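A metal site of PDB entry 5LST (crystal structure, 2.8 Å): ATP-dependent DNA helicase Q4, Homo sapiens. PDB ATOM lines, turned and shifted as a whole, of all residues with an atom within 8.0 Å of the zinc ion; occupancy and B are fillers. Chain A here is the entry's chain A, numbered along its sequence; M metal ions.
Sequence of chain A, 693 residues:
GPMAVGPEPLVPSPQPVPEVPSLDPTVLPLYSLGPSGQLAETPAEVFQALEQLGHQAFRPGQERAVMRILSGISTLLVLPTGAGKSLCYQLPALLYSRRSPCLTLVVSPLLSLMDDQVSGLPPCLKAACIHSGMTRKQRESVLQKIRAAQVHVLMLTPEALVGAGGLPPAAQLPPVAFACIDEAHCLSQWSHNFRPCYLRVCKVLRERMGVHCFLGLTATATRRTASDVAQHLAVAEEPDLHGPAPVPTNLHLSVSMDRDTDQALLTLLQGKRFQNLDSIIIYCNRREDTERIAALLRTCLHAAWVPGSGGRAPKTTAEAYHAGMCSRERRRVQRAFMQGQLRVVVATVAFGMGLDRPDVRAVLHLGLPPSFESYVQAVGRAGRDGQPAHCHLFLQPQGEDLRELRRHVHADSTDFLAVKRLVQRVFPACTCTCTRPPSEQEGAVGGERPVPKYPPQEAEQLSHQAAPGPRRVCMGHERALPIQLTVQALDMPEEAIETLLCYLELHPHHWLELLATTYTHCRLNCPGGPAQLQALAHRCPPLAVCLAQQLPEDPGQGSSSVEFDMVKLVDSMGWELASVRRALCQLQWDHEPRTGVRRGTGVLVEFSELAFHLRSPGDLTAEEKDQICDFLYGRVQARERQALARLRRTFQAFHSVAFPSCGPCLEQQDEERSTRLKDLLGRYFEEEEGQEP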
ATOM      1  N   PRO A 428     -22.341   2.894  20.307  1.00  0.00           N
ATOM      2  CA  PRO A 428     -21.660   4.185  20.443  1.00  0.00           C
ATOM      3  C   PRO A 428     -22.635   5.266  20.874  1.00  0.00           C
ATOM      4  O   PRO A 428     -23.836   5.196  20.603  1.00  0.00           O
ATOM      5  CB  PRO A 428     -21.106   4.451  19.044  1.00  0.00           C
ATOM      6  CG  PRO A 428     -21.642   3.346  18.155  1.00  0.00           C
ATOM      7  CD  PRO A 428     -22.705   2.633  18.906  1.00  0.00           C
ATOM      8  N   ALA A 429     -22.103   6.299  21.535  1.00  0.00           N
ATOM      9  CA  ALA A 429     -22.934   7.368  22.059  1.00  0.00           C
ATOM     10  C   ALA A 429     -23.536   8.201  20.934  1.00  0.00           C
ATOM     11  O   ALA A 429     -22.913   8.417  19.888  1.00  0.00           O
ATOM     12  CB  ALA A 429     -22.124   8.268  22.994  1.00  0.00           C
ATOM     13  N   CYS A 430     -24.756   8.675  21.148  1.00  0.00           N
ATOM     14  CA  CYS A 430     -25.463   9.535  20.204  1.00  0.00           C
ATOM     15  C   CYS A 430     -25.646  10.928  20.807  1.00  0.00           C
ATOM     16  O   CYS A 430     -25.406  11.163  21.993  1.00  0.00           O
ATOM     17  CB  CYS A 430     -26.813   8.936  19.798  1.00  0.00           C
ATOM     18  SG  CYS A 430     -28.076   8.977  21.094  1.00  0.00           S
ATOM     19  N   THR A 431     -26.098  11.858  19.959  1.00  0.00           N
ATOM     20  CA  THR A 431     -26.280  13.250  20.339  1.00  0.00           C
ATOM     21  C   THR A 431     -27.726  13.564  20.742  1.00  0.00           C
ATOM     22  O   THR A 431     -28.109  14.740  20.765  1.00  0.00           O
ATOM     23  CB  THR A 431     -25.834  14.169  19.201  1.00  0.00           C
ATOM     24  OG1 THR A 431     -26.532  13.825  18.005  1.00  0.00           O
ATOM     25  CG2 THR A 431     -24.336  14.030  18.968  1.00  0.00           C
ATOM     26  N   CYS A 432     -28.526  12.547  21.061  1.00  0.00           N
ATOM     27  CA  CYS A 432     -29.916  12.797  21.433  1.00  0.00           C
ATOM     28  C   CYS A 432     -30.028  13.435  22.822  1.00  0.00           C
ATOM     29  O   CYS A 432     -30.959  14.206  23.059  1.00  0.00           O
ATOM     30  CB  CYS A 432     -30.731  11.498  21.381  1.00  0.00           C
ATOM     31  SG  CYS A 432     -30.963  10.753  19.747  1.00  0.00           S
ATOM     32  N   THR A 433     -29.104  13.125  23.725  1.00  0.00           N
ATOM     33  CA  THR A 433     -29.091  13.714  25.065  1.00  0.00           C
ATOM     34  C   THR A 433     -27.712  14.285  25.398  1.00  0.00           C
ATOM     35  O   THR A 433     -27.266  14.217  26.540  1.00  0.00           O
ATOM     36  CB  THR A 433     -29.534  12.707  26.123  1.00  0.00           C
ATOM     37  OG1 THR A 433     -30.538  11.847  25.574  1.00  0.00           O
ATOM     38  CG2 THR A 433     -30.127  13.427  27.335  1.00  0.00           C
ATOM     39  N   ARG A 472     -33.683  14.932  23.497  1.00  0.00           N
ATOM     40  CA  ARG A 472     -34.746  14.007  23.137  1.00  0.00           C
ATOM     41  C   ARG A 472     -34.475  12.645  23.763  1.00  0.00           C
ATOM     42  O   ARG A 472     -33.372  12.347  24.210  1.00  0.00           O
ATOM     43  CB  ARG A 472     -34.884  13.853  21.617  1.00  0.00           C
ATOM     44  CG  ARG A 472     -35.016  15.153  20.845  1.00  0.00           C
ATOM     45  CD  ARG A 472     -36.269  15.923  21.221  1.00  0.00           C
ATOM     46  NE  ARG A 472     -37.502  15.160  21.014  1.00  0.00           N
ATOM     47  CZ  ARG A 472     -38.092  15.007  19.840  1.00  0.00           C
ATOM     48  NH1 ARG A 472     -37.571  15.545  18.744  1.00  0.00           N
ATOM     49  NH2 ARG A 472     -39.217  14.308  19.749  1.00  0.00           N
ATOM     50  N   VAL A 473     -35.503  11.812  23.754  1.00  0.00           N
ATOM     51  CA  VAL A 473     -35.385  10.413  24.164  1.00  0.00           C
ATOM     52  C   VAL A 473     -34.975   9.610  22.941  1.00  0.00           C
ATOM     53  O   VAL A 473     -35.644   9.633  21.907  1.00  0.00           O
ATOM     54  CB  VAL A 473     -36.698   9.895  24.756  1.00  0.00           C
ATOM     55  CG1 VAL A 473     -36.596   8.407  25.030  1.00  0.00           C
ATOM     56  CG2 VAL A 473     -37.038  10.650  26.029  1.00  0.00           C
ATOM     57  N   CYS A 474     -33.857   8.893  23.056  1.00  0.00           N
ATOM     58  CA  CYS A 474     -33.266   8.202  21.914  1.00  0.00           C
ATOM     59  C   CYS A 474     -34.208   7.101  21.411  1.00  0.00           C
ATOM     60  O   CYS A 474     -34.589   6.199  22.171  1.00  0.00           O
ATOM     61  CB  CYS A 474     -31.916   7.615  22.303  1.00  0.00           C
ATOM     62  SG  CYS A 474     -31.059   6.770  20.972  1.00  0.00           S
ATOM     63  N   MET A 475     -34.573   7.163  20.138  1.00  0.00           N
ATOM     64  CA  MET A 475     -35.431   6.179  19.503  1.00  0.00           C
ATOM     65  C   MET A 475     -34.637   5.134  18.727  1.00  0.00           C
ATOM     66  O   MET A 475     -35.195   4.462  17.851  1.00  0.00           O
ATOM     67  CB  MET A 475     -36.441   6.865  18.587  1.00  0.00           C
ATOM     68  CG  MET A 475     -37.266   7.928  19.260  1.00  0.00           C
ATOM     69  SD  MET A 475     -38.258   7.247  20.593  1.00  0.00           S
ATOM     70  CE  MET A 475     -39.129   8.712  21.161  1.00  0.00           C
ATOM     71  N   GLY A 476     -33.362   4.979  19.018  1.00  0.00           N
ATOM     72  CA  GLY A 476     -32.519   4.017  18.352  1.00  0.00           C
ATOM     73  C   GLY A 476     -31.863   4.583  17.111  1.00  0.00           C
ATOM     74  O   GLY A 476     -32.316   5.552  16.507  1.00  0.00           O
ATOM     75  N   HIS A 477     -30.760   3.956  16.716  1.00  0.00           N
ATOM     76  CA  HIS A 477     -30.035   4.313  15.519  1.00  0.00           C
ATOM     77  C   HIS A 477     -29.666   3.053  14.754  1.00  0.00           C
ATOM     78  O   HIS A 477     -29.417   2.001  15.342  1.00  0.00           O
ATOM     79  CB  HIS A 477     -28.773   5.129  15.827  1.00  0.00           C
ATOM     80  CG  HIS A 477     -29.046   6.364  16.628  1.00  0.00           C
ATOM     81  ND1 HIS A 477     -29.365   7.567  16.038  1.00  0.00           N
ATOM     82  CD2 HIS A 477     -29.062   6.577  17.964  1.00  0.00           C
ATOM     83  CE1 HIS A 477     -29.563   8.474  16.984  1.00  0.00           C
ATOM     84  NE2 HIS A 477     -29.386   7.897  18.158  1.00  0.00           N
ATOM     85  N   ARG A 479     -26.959   1.219  12.397  1.00  0.00           N
ATOM     86  CA  ARG A 479     -25.524   1.277  12.190  1.00  0.00           C
ATOM     87  C   ARG A 479     -25.082   0.159  11.262  1.00  0.00           C
ATOM     88  O   ARG A 479     -25.717  -0.898  11.185  1.00  0.00           O
ATOM     89  CB  ARG A 479     -24.761   1.164  13.510  1.00  0.00           C
ATOM     90  CG  ARG A 479     -25.431   1.874  14.655  1.00  0.00           C
ATOM     91  CD  ARG A 479     -24.749   1.588  15.967  1.00  0.00           C
ATOM     92  NE  ARG A 479     -25.554   2.076  17.088  1.00  0.00           N
ATOM     93  CZ  ARG A 479     -25.666   3.347  17.411  1.00  0.00           C
ATOM     94  NH1 ARG A 479     -25.032   4.275  16.710  1.00  0.00           N
ATOM     95  NH2 ARG A 479     -26.417   3.698  18.445  1.00  0.00           N
ATOM     96  N   ASP A 571     -29.747   6.975   8.916  1.00  0.00           N
ATOM     97  CA  ASP A 571     -30.087   7.466  10.244  1.00  0.00           C
ATOM     98  C   ASP A 571     -30.270   8.982  10.264  1.00  0.00           C
ATOM     99  O   ASP A 571     -31.140   9.476  10.988  1.00  0.00           O
ATOM    100  CB  ASP A 571     -28.995   7.072  11.246  1.00  0.00           C
ATOM    101  CG  ASP A 571     -29.397   7.363  12.668  1.00  0.00           C
ATOM    102  OD1 ASP A 571     -30.313   6.685  13.180  1.00  0.00           O
ATOM    103  OD2 ASP A 571     -28.795   8.286  13.274  1.00  0.00           O
ATOM    104  N   SER A 616     -29.476  -0.192  17.485  1.00  0.00           N
ATOM    105  CA  SER A 616     -29.157  -0.179  18.905  1.00  0.00           C
ATOM    106  C   SER A 616     -29.324   1.234  19.460  1.00  0.00           C
ATOM    107  O   SER A 616     -29.164   2.218  18.728  1.00  0.00           O
ATOM    108  CB  SER A 616     -27.724  -0.659  19.160  1.00  0.00           C
ATOM    109  OG  SER A 616     -26.798   0.104  18.395  1.00  0.00           O
ATOM    110  N   PRO A 617     -29.639   1.357  20.752  1.00  0.00           N
ATOM    111  CA  PRO A 617     -29.721   2.692  21.350  1.00  0.00           C
ATOM    112  C   PRO A 617     -28.352   3.346  21.439  1.00  0.00           C
ATOM    113  O   PRO A 617     -27.311   2.680  21.433  1.00  0.00           O
ATOM    114  CB  PRO A 617     -30.288   2.405  22.746  1.00  0.00           C
ATOM    115  CG  PRO A 617     -29.846   1.022  23.049  1.00  0.00           C
ATOM    116  CD  PRO A 617     -29.887   0.286  21.737  1.00  0.00           C
ATOM    117  N   GLY A 618     -28.372   4.670  21.533  1.00  0.00           N
ATOM    118  CA  GLY A 618     -27.137   5.424  21.674  1.00  0.00           C
ATOM    119  C   GLY A 618     -26.993   6.117  23.012  1.00  0.00           C
ATOM    120  O   GLY A 618     -26.086   6.940  23.182  1.00  0.00           O
ATOM    121  N   ASP A 619     -27.861   5.807  23.979  1.00  0.00           N
ATOM    122  CA  ASP A 619     -27.893   6.506  25.263  1.00  0.00           C
ATOM    123  C   ASP A 619     -27.443   5.633  26.424  1.00  0.00           C
ATOM    124  O   ASP A 619     -27.734   5.952  27.588  1.00  0.00           O
ATOM    125  CB  ASP A 619     -29.296   7.048  25.535  1.00  0.00           C
ATOM    126  CG  ASP A 619     -30.332   5.947  25.718  1.00  0.00           C
ATOM    127  OD1 ASP A 619     -30.110   4.826  25.187  1.00  0.00           O
ATOM    128  OD2 ASP A 619     -31.346   6.193  26.392  1.00  0.00           O
HETATM  129 ZN    ZN M   1     -30.032   8.575  19.952  1.00  0.00          ZN
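The backbone carbonyl oxygen (O) of His 477 is in hydrogen-bond range of the backbone NH (N) of Ser 616 (3.1 Å).
The side-chain carboxylate (OD2) of Asp 571 lies within hydrogen-bond range of a ring nitrogen (ND1) of His 477, at 2.9 Å.
The backbone carbonyl oxygen of Gly 618 sits at hydrogen-bond distance from the backbone NH of Cys 430, 3.0 Å away.
The side-chain sulfur (SG) of Cys 474 lies close to the backbone NH (N) of Gly 618, at 3.5 Å.
SG of Cys 474 lies close to N of Gly 476, 3.5 Å away.
O of Cys 432 sits at hydrogen-bond distance from N of Arg 472 (2.9 Å).
Four residues have an atom within 4 Å of the zinc ion: Cys 430, Cys 432, Cys 474 and His 477.
The nearest printed residue that does not touch the zinc ion is Gly 618 (4.5 Å).
NE2 of His 477 is bound to the zinc ion (2.0 Å).
The zinc ion is bound by the side-chain sulfur (SG) of Cys 430 (2.3 Å).
SG of Cys 474 is bound to the zinc ion, 2.3 Å away.
The zinc ion is bound by the side-chain sulfur (SG) of Cys 432.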
